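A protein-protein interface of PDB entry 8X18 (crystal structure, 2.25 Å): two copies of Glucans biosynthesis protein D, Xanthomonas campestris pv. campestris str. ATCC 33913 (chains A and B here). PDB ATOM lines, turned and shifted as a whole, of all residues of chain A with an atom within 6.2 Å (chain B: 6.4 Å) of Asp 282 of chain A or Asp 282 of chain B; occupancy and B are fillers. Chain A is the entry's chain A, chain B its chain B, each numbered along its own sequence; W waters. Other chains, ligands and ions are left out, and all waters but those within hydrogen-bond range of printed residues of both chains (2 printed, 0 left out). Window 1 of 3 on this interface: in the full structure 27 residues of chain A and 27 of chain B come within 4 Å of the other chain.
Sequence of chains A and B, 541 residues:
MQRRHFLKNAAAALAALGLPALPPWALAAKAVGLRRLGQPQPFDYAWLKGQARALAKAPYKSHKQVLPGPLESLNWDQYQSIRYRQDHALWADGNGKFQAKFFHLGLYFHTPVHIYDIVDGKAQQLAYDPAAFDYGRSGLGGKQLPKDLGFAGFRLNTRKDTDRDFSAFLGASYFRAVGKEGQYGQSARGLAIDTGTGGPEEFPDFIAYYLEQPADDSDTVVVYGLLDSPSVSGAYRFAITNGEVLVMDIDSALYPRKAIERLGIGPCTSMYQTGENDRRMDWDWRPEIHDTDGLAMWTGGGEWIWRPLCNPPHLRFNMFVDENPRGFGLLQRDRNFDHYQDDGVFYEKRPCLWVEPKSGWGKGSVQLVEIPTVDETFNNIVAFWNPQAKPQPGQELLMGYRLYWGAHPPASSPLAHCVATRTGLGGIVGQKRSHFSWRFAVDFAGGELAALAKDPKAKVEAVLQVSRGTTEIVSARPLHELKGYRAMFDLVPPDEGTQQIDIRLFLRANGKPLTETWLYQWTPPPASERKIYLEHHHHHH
Printed residues of chain B that touch a printed residue of chain A: Asp 282, Trp 283, Asp 284, Trp 285, Thr 423 and Gly 424.
Among the printed residues, 10 pairs touch across the chains.
Among the printed residues, no Asp or Glu carboxylate lies within 4 Å of a Lys or Arg side-chain nitrogen of the other chain.
The backbone carbonyl oxygen (O) of Asp 282 of chain B lies within hydrogen-bond range of the guanidinium group (NH1) of Arg 279 of chain A.
O of Asp 284 of chain B sits at hydrogen-bond distance from NH2 of Arg 279 of chain A (3.1 Å).
OD2 of Asp 282 of chain B sits close to OD2 of Asp 282 of chain A (2.7 Å).
Water W2 lies within hydrogen-bond range of NE of Arg 279 of chain B (2.9 Å) and O of Asp 284 of chain A (3.0 Å).
Water W1 bridges the backbone carbonyl oxygen (O) of Thr 423 of chain B (3.3 Å) and the backbone carbonyl oxygen (O) of Asp 284 of chain A (3.4 Å).
The backbone carbonyl oxygen of Thr 423 of chain A is in hydrogen-bond range of the guanidinium group of Arg 279 of chain A.
Asp 282 of chain A touches just one residue of chain B: Asp 282.
Of the printed residues of chain A, Trp 283 of chain B touches Arg 279 and Gly 424.
Of the printed residues of chain B, Trp 283 of chain A touches Gly 424 (3.4 Å).
Printed residues of chain B within 4 Å of Gly 424 of chain A: Trp 283 (3.1 Å), Asp 284 (3.9 Å) and Trp 285 (3.7 Å).
Of the printed residues of chain A, Thr 423 of chain B touches Asp 284 (3.8 Å).
Of the printed residues of chain A, Trp 285 of chain B touches Thr 423 and Gly 424.
Asp 278 of chain B touches none of the printed residues of chain A.
Thr 274 of chain B touches none of the printed residues of chain A.
The nearest residue of chain B that does not touch Asp 282 of chain A is Arg 279 of chain B (5.4 Å).
The nearest printed residue of chain A that does not touch Asp 282 of chain B is Gly 424 of chain A (6.0 Å).
Arg 279 of chain A touches Asp 282 of chain B, but with the chains exchanged Asp 282 of chain A does not touch Arg 279 of chain B (5.4 Å).
Arg 279 of chain A touches Asp 284 of chain B, but with the chains exchanged Asp 284 of chain A does not touch Arg 279 of chain B (5.5 Å).
Trp 283 of chain A touches Gly 424 of chain B, and with the chains exchanged Gly 424 of chain A touches Trp 283 of chain B.
Gly 424 of chain A touches Asp 284 of chain B, but with the chains exchanged Asp 284 of chain A does not touch Gly 424 of chain B (4.1 Å).
Of the 10 pairs that touch across the chains among the printed residues, 3 have their exchanged pair printed and touching as well.
Among the printed residues, merely in contact across the chains: Gly 424 of chain A with Trp 283 of chain B (3.1 Å), Thr 423 of chain A with Trp 285 of chain B (3.4 Å), Trp 283 of chain A with Gly 424 of chain B (3.4 Å), Gly 424 of chain A with Trp 285 of chain B (3.7 Å), Asp 284 of chain A with Thr 423 of chain B (3.8 Å), Arg 279 of chain A with Trp 283 of chain B (3.9 Å) and Gly 424 of chain A with Asp 284 of chain B (3.9 Å).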
ATOM      1  N   GLN A 273      -6.627 -12.176   3.924  1.00  0.00           N
ATOM      2  CA  GLN A 273      -8.060 -12.315   3.712  1.00  0.00           C
ATOM      3  C   GLN A 273      -8.549 -13.687   4.165  1.00  0.00           C
ATOM      4  O   GLN A 273      -9.582 -13.803   4.843  1.00  0.00           O
ATOM      5  CB  GLN A 273      -8.453 -12.084   2.255  1.00  0.00           C
ATOM      6  CG  GLN A 273      -9.970 -12.209   2.021  1.00  0.00           C
ATOM      7  CD  GLN A 273     -10.335 -12.144   0.562  1.00  0.00           C
ATOM      8  OE1 GLN A 273      -9.759 -11.387  -0.211  1.00  0.00           O
ATOM      9  NE2 GLN A 273     -11.278 -12.974   0.157  1.00  0.00           N
ATOM     10  N   THR A 274      -7.914 -14.739   3.668  1.00  0.00           N
ATOM     11  CA  THR A 274      -8.444 -16.078   3.911  1.00  0.00           C
ATOM     12  C   THR A 274      -7.335 -17.086   3.683  1.00  0.00           C
ATOM     13  O   THR A 274      -6.358 -16.821   2.982  1.00  0.00           O
ATOM     14  CB  THR A 274      -9.628 -16.403   2.984  1.00  0.00           C
ATOM     15  OG1 THR A 274     -10.275 -17.592   3.415  1.00  0.00           O
ATOM     16  CG2 THR A 274      -9.215 -16.569   1.536  1.00  0.00           C
ATOM     17  N   ASP A 278      -7.693 -19.379   8.837  1.00  0.00           N
ATOM     18  CA  ASP A 278      -8.986 -18.750   9.090  1.00  0.00           C
ATOM     19  C   ASP A 278      -9.772 -18.620   7.782  1.00  0.00           C
ATOM     20  O   ASP A 278      -9.445 -17.779   6.920  1.00  0.00           O
ATOM     21  CB  ASP A 278      -8.783 -17.357   9.719  1.00  0.00           C
ATOM     22  CG  ASP A 278     -10.068 -16.640  10.080  1.00  0.00           C
ATOM     23  OD1 ASP A 278     -11.163 -17.275   9.892  1.00  0.00           O
ATOM     24  OD2 ASP A 278      -9.975 -15.463  10.557  1.00  0.00           O
ATOM     25  N   ARG A 279     -10.851 -19.413   7.697  1.00  0.00           N
ATOM     26  CA  ARG A 279     -11.673 -19.549   6.508  1.00  0.00           C
ATOM     27  C   ARG A 279     -12.965 -18.729   6.610  1.00  0.00           C
ATOM     28  O   ARG A 279     -13.879 -18.879   5.798  1.00  0.00           O
ATOM     29  CB  ARG A 279     -11.964 -21.040   6.287  1.00  0.00           C
ATOM     30  CG  ARG A 279     -10.760 -21.847   5.824  1.00  0.00           C
ATOM     31  CD  ARG A 279     -10.953 -23.366   5.676  1.00  0.00           C
ATOM     32  NE  ARG A 279     -11.389 -24.093   6.891  1.00  0.00           N
ATOM     33  CZ  ARG A 279     -12.645 -24.501   7.140  1.00  0.00           C
ATOM     34  NH1 ARG A 279     -13.629 -24.327   6.260  1.00  0.00           N
ATOM     35  NH2 ARG A 279     -12.933 -25.067   8.298  1.00  0.00           N
ATOM     36  N   ARG A 280     -13.070 -17.829   7.589  1.00  0.00           N
ATOM     37  CA  ARG A 280     -14.270 -17.007   7.738  1.00  0.00           C
ATOM     38  C   ARG A 280     -14.654 -16.313   6.429  1.00  0.00           C
ATOM     39  O   ARG A 280     -15.823 -16.303   6.073  1.00  0.00           O
ATOM     40  CB  ARG A 280     -14.051 -15.927   8.808  1.00  0.00           C
ATOM     41  CG  ARG A 280     -15.317 -15.232   9.292  1.00  0.00           C
ATOM     42  CD  ARG A 280     -15.072 -14.131  10.343  1.00  0.00           C
ATOM     43  NE  ARG A 280     -14.245 -13.009   9.867  1.00  0.00           N
ATOM     44  CZ  ARG A 280     -14.639 -12.003   9.081  1.00  0.00           C
ATOM     45  NH1 ARG A 280     -15.911 -11.862   8.774  1.00  0.00           N
ATOM     46  NH2 ARG A 280     -13.774 -11.098   8.632  1.00  0.00           N
ATOM     47  N   MET A 281     -13.693 -15.687   5.767  1.00  0.00           N
ATOM     48  CA  MET A 281     -13.960 -15.008   4.481  1.00  0.00           C
ATOM     49  C   MET A 281     -13.457 -15.875   3.320  1.00  0.00           C
ATOM     50  O   MET A 281     -12.651 -15.376   2.531  1.00  0.00           O
ATOM     51  CB  MET A 281     -13.310 -13.623   4.456  1.00  0.00           C
ATOM     52  CG  MET A 281     -14.112 -12.569   5.185  1.00  0.00           C
ATOM     53  SD  MET A 281     -15.650 -12.151   4.334  1.00  0.00           S
ATOM     54  CE  MET A 281     -16.843 -12.601   5.589  1.00  0.00           C
ATOM     55  N   ASP A 282     -13.972 -17.096   3.198  1.00  0.00           N
ATOM     56  CA  ASP A 282     -13.609 -18.003   2.075  1.00  0.00           C
ATOM     57  C   ASP A 282     -14.606 -17.823   0.918  1.00  0.00           C
ATOM     58  O   ASP A 282     -15.244 -18.794   0.540  1.00  0.00           O
ATOM     59  CB  ASP A 282     -13.489 -19.442   2.584  1.00  0.00           C
ATOM     60  CG  ASP A 282     -14.780 -20.009   3.151  1.00  0.00           C
ATOM     61  OD1 ASP A 282     -15.774 -19.262   3.232  1.00  0.00           O
ATOM     62  OD2 ASP A 282     -14.779 -21.195   3.511  1.00  0.00           O
ATOM     63  N   TRP A 283     -14.701 -16.619   0.365  1.00  0.00           N
ATOM     64  CA  TRP A 283     -15.660 -16.297  -0.720  1.00  0.00           C
ATOM     65  C   TRP A 283     -14.990 -16.398  -2.085  1.00  0.00           C
ATOM     66  O   TRP A 283     -15.677 -16.189  -3.072  1.00  0.00           O
ATOM     67  CB  TRP A 283     -16.148 -14.861  -0.523  1.00  0.00           C
ATOM     68  CG  TRP A 283     -17.050 -14.591   0.636  1.00  0.00           C
ATOM     69  CD1 TRP A 283     -17.457 -15.458   1.606  1.00  0.00           C
ATOM     70  CD2 TRP A 283     -17.664 -13.330   0.938  1.00  0.00           C
ATOM     71  NE1 TRP A 283     -18.287 -14.822   2.486  1.00  0.00           N
ATOM     72  CE2 TRP A 283     -18.433 -13.516   2.103  1.00  0.00           C
ATOM     73  CE3 TRP A 283     -17.643 -12.069   0.336  1.00  0.00           C
ATOM     74  CZ2 TRP A 283     -19.170 -12.482   2.675  1.00  0.00           C
ATOM     75  CZ3 TRP A 283     -18.374 -11.049   0.901  1.00  0.00           C
ATOM     76  CH2 TRP A 283     -19.125 -11.257   2.055  1.00  0.00           C
ATOM     77  N   ASP A 284     -13.705 -16.704  -2.131  1.00  0.00           N
ATOM     78  CA  ASP A 284     -12.978 -16.643  -3.379  1.00  0.00           C
ATOM     79  C   ASP A 284     -12.741 -18.062  -3.888  1.00  0.00           C
ATOM     80  O   ASP A 284     -12.735 -19.004  -3.101  1.00  0.00           O
ATOM     81  CB  ASP A 284     -11.656 -15.889  -3.191  1.00  0.00           C
ATOM     82  CG  ASP A 284     -11.128 -15.243  -4.456  1.00  0.00           C
ATOM     83  OD1 ASP A 284     -10.531 -15.973  -5.285  1.00  0.00           O
ATOM     84  OD2 ASP A 284     -11.360 -14.027  -4.619  1.00  0.00           O
ATOM     85  N   THR A 423      -8.325 -25.742  10.930  1.00  0.00           N
ATOM     86  CA  THR A 423      -9.332 -25.767  11.968  1.00  0.00           C
ATOM     87  C   THR A 423     -10.714 -26.021  11.362  1.00  0.00           C
ATOM     88  O   THR A 423     -10.965 -25.705  10.214  1.00  0.00           O
ATOM     89  CB  THR A 423      -9.322 -24.481  12.815  1.00  0.00           C
ATOM     90  OG1 THR A 423     -10.292 -23.635  12.210  1.00  0.00           O
ATOM     91  CG2 THR A 423      -7.973 -23.796  12.886  1.00  0.00           C
ATOM     92  N   GLY A 424     -11.614 -26.566  12.179  1.00  0.00           N
ATOM     93  CA  GLY A 424     -12.962 -26.910  11.774  1.00  0.00           C
ATOM     94  C   GLY A 424     -13.768 -27.362  12.994  1.00  0.00           C
ATOM     95  O   GLY A 424     -13.284 -27.319  14.130  1.00  0.00           O
ATOM     96  N   GLN B 273     -18.738 -34.703   0.484  1.00  0.00           N
ATOM     97  CA  GLN B 273     -19.108 -33.755   1.509  1.00  0.00           C
ATOM     98  C   GLN B 273     -18.657 -32.343   1.147  1.00  0.00           C
ATOM     99  O   GLN B 273     -19.439 -31.399   1.311  1.00  0.00           O
ATOM    100  CB  GLN B 273     -18.538 -34.108   2.868  1.00  0.00           C
ATOM    101  CG  GLN B 273     -18.821 -33.018   3.904  1.00  0.00           C
ATOM    102  CD  GLN B 273     -18.400 -33.421   5.299  1.00  0.00           C
ATOM    103  OE1 GLN B 273     -18.480 -34.572   5.716  1.00  0.00           O
ATOM    104  NE2 GLN B 273     -17.937 -32.455   6.063  1.00  0.00           N
ATOM    105  N   THR B 274     -17.383 -32.181   0.811  1.00  0.00           N
ATOM    106  CA  THR B 274     -16.855 -30.855   0.544  1.00  0.00           C
ATOM    107  C   THR B 274     -15.589 -30.980  -0.298  1.00  0.00           C
ATOM    108  O   THR B 274     -14.945 -32.026  -0.308  1.00  0.00           O
ATOM    109  CB  THR B 274     -16.579 -30.109   1.861  1.00  0.00           C
ATOM    110  OG1 THR B 274     -16.365 -28.726   1.572  1.00  0.00           O
ATOM    111  CG2 THR B 274     -15.364 -30.658   2.585  1.00  0.00           C
ATOM    112  N   ASP B 278     -17.283 -27.607  -4.567  1.00  0.00           N
ATOM    113  CA  ASP B 278     -18.443 -27.157  -3.839  1.00  0.00           C
ATOM    114  C   ASP B 278     -18.085 -27.089  -2.358  1.00  0.00           C
ATOM    115  O   ASP B 278     -18.099 -28.128  -1.679  1.00  0.00           O
ATOM    116  CB  ASP B 278     -19.654 -28.086  -4.039  1.00  0.00           C
ATOM    117  CG  ASP B 278     -20.906 -27.575  -3.345  1.00  0.00           C
ATOM    118  OD1 ASP B 278     -20.873 -26.435  -2.741  1.00  0.00           O
ATOM    119  OD2 ASP B 278     -21.907 -28.271  -3.439  1.00  0.00           O
ATOM    120  N   ARG B 279     -17.887 -25.876  -1.870  1.00  0.00           N
ATOM    121  CA  ARG B 279     -17.454 -25.669  -0.471  1.00  0.00           C
ATOM    122  C   ARG B 279     -18.648 -25.242   0.397  1.00  0.00           C
ATOM    123  O   ARG B 279     -18.415 -24.685   1.463  1.00  0.00           O
ATOM    124  CB  ARG B 279     -16.310 -24.649  -0.479  1.00  0.00           C
ATOM    125  CG  ARG B 279     -14.937 -25.190  -0.859  1.00  0.00           C
ATOM    126  CD  ARG B 279     -14.026 -24.199  -1.575  1.00  0.00           C
ATOM    127  NE  ARG B 279     -12.579 -24.241  -1.331  1.00  0.00           N
ATOM    128  CZ  ARG B 279     -11.811 -25.320  -1.465  1.00  0.00           C
ATOM    129  NH1 ARG B 279     -12.118 -26.443  -0.840  1.00  0.00           N
ATOM    130  NH2 ARG B 279     -10.728 -25.269  -2.221  1.00  0.00           N
ATOM    131  N   ARG B 280     -19.878 -25.516  -0.043  1.00  0.00           N
ATOM    132  CA  ARG B 280     -21.053 -25.131   0.730  1.00  0.00           C
ATOM    133  C   ARG B 280     -20.936 -25.682   2.150  1.00  0.00           C
ATOM    134  O   ARG B 280     -21.204 -24.982   3.100  1.00  0.00           O
ATOM    135  CB  ARG B 280     -22.345 -25.666   0.097  1.00  0.00           C
ATOM    136  CG  ARG B 280     -23.623 -25.192   0.794  1.00  0.00           C
ATOM    137  CD  ARG B 280     -24.905 -25.728   0.184  1.00  0.00           C
ATOM    138  NE  ARG B 280     -24.992 -27.177   0.358  1.00  0.00           N
ATOM    139  CZ  ARG B 280     -25.370 -27.778   1.457  1.00  0.00           C
ATOM    140  NH1 ARG B 280     -25.846 -27.065   2.454  1.00  0.00           N
ATOM    141  NH2 ARG B 280     -25.314 -29.084   1.564  1.00  0.00           N
ATOM    142  N   MET B 281     -20.563 -26.947   2.305  1.00  0.00           N
ATOM    143  CA  MET B 281     -20.416 -27.524   3.626  1.00  0.00           C
ATOM    144  C   MET B 281     -18.929 -27.618   4.013  1.00  0.00           C
ATOM    145  O   MET B 281     -18.378 -28.689   4.181  1.00  0.00           O
ATOM    146  CB  MET B 281     -21.081 -28.902   3.679  1.00  0.00           C
ATOM    147  CG  MET B 281     -20.954 -29.536   5.063  1.00  0.00           C
ATOM    148  SD  MET B 281     -22.159 -28.890   6.288  1.00  0.00           S
ATOM    149  CE  MET B 281     -23.395 -28.012   5.318  1.00  0.00           C
ATOM    150  N   ASP B 282     -18.339 -26.472   4.334  1.00  0.00           N
ATOM    151  CA  ASP B 282     -16.901 -26.378   4.702  1.00  0.00           C
ATOM    152  C   ASP B 282     -16.678 -26.353   6.219  1.00  0.00           C
ATOM    153  O   ASP B 282     -15.879 -25.546   6.681  1.00  0.00           O
ATOM    154  CB  ASP B 282     -16.352 -25.072   4.136  1.00  0.00           C
ATOM    155  CG  ASP B 282     -17.182 -23.859   4.522  1.00  0.00           C
ATOM    156  OD1 ASP B 282     -18.078 -23.992   5.374  1.00  0.00           O
ATOM    157  OD2 ASP B 282     -16.931 -22.794   3.962  1.00  0.00           O
ATOM    158  N   TRP B 283     -17.350 -27.217   6.959  1.00  0.00           N
ATOM    159  CA  TRP B 283     -17.252 -27.166   8.404  1.00  0.00           C
ATOM    160  C   TRP B 283     -15.938 -27.765   8.901  1.00  0.00           C
ATOM    161  O   TRP B 283     -15.495 -27.451   9.995  1.00  0.00           O
ATOM    162  CB  TRP B 283     -18.451 -27.905   9.007  1.00  0.00           C
ATOM    163  CG  TRP B 283     -19.723 -27.143   8.836  1.00  0.00           C
ATOM    164  CD1 TRP B 283     -19.886 -25.958   8.178  1.00  0.00           C
ATOM    165  CD2 TRP B 283     -21.008 -27.490   9.359  1.00  0.00           C
ATOM    166  NE1 TRP B 283     -21.187 -25.555   8.259  1.00  0.00           N
ATOM    167  CE2 TRP B 283     -21.899 -26.472   8.976  1.00  0.00           C
ATOM    168  CE3 TRP B 283     -21.488 -28.567  10.104  1.00  0.00           C
ATOM    169  CZ2 TRP B 283     -23.245 -26.486   9.327  1.00  0.00           C
ATOM    170  CZ3 TRP B 283     -22.813 -28.584  10.459  1.00  0.00           C
ATOM    171  CH2 TRP B 283     -23.675 -27.555  10.078  1.00  0.00           C
ATOM    172  N   ASP B 284     -15.331 -28.630   8.106  1.00  0.00           N
ATOM    173  CA  ASP B 284     -14.299 -29.523   8.580  1.00  0.00           C
ATOM    174  C   ASP B 284     -12.951 -28.858   8.347  1.00  0.00           C
ATOM    175  O   ASP B 284     -12.833 -28.021   7.456  1.00  0.00           O
ATOM    176  CB  ASP B 284     -14.354 -30.864   7.851  1.00  0.00           C
ATOM    177  CG  ASP B 284     -13.687 -31.991   8.611  1.00  0.00           C
ATOM    178  OD1 ASP B 284     -12.432 -32.017   8.644  1.00  0.00           O
ATOM    179  OD2 ASP B 284     -14.423 -32.758   9.226  1.00  0.00           O
ATOM    180  N   TRP B 285     -11.957 -29.263   9.150  1.00  0.00           N
ATOM    181  CA  TRP B 285     -10.592 -28.820   8.942  1.00  0.00           C
ATOM    182  C   TRP B 285      -9.996 -29.425   7.672  1.00  0.00           C
ATOM    183  O   TRP B 285      -9.002 -28.917   7.160  1.00  0.00           O
ATOM    184  CB  TRP B 285      -9.717 -29.140  10.168  1.00  0.00           C
ATOM    185  CG  TRP B 285      -9.442 -30.587  10.444  1.00  0.00           C
ATOM    186  CD1 TRP B 285     -10.153 -31.420  11.260  1.00  0.00           C
ATOM    187  CD2 TRP B 285      -8.359 -31.373   9.945  1.00  0.00           C
ATOM    188  NE1 TRP B 285      -9.624 -32.685  11.250  1.00  0.00           N
ATOM    189  CE2 TRP B 285      -8.497 -32.675  10.478  1.00  0.00           C
ATOM    190  CE3 TRP B 285      -7.288 -31.112   9.107  1.00  0.00           C
ATOM    191  CZ2 TRP B 285      -7.589 -33.697  10.224  1.00  0.00           C
ATOM    192  CZ3 TRP B 285      -6.408 -32.130   8.833  1.00  0.00           C
ATOM    193  CH2 TRP B 285      -6.566 -33.411   9.363  1.00  0.00           C
ATOM    194  N   THR B 423     -14.480 -22.313  -7.539  1.00  0.00           N
ATOM    195  CA  THR B 423     -15.537 -21.347  -7.743  1.00  0.00           C
ATOM    196  C   THR B 423     -15.536 -20.370  -6.583  1.00  0.00           C
ATOM    197  O   THR B 423     -15.056 -20.714  -5.515  1.00  0.00           O
ATOM    198  CB  THR B 423     -16.926 -21.993  -7.873  1.00  0.00           C
ATOM    199  OG1 THR B 423     -17.499 -22.193  -6.589  1.00  0.00           O
ATOM    200  CG2 THR B 423     -16.897 -23.332  -8.557  1.00  0.00           C
ATOM    201  N   GLY B 424     -16.122 -19.189  -6.794  1.00  0.00           N
ATOM    202  CA  GLY B 424     -16.356 -18.239  -5.707  1.00  0.00           C
ATOM    203  C   GLY B 424     -17.098 -16.993  -6.193  1.00  0.00           C
ATOM    204  O   GLY B 424     -17.509 -16.937  -7.355  1.00  0.00           O
HETATM  205  O   HOH W   1     -14.892 -21.550  -2.372  1.00  0.00           O
HETATM  206  O   HOH W   2     -11.707 -21.583  -2.005  1.00  0.00           O
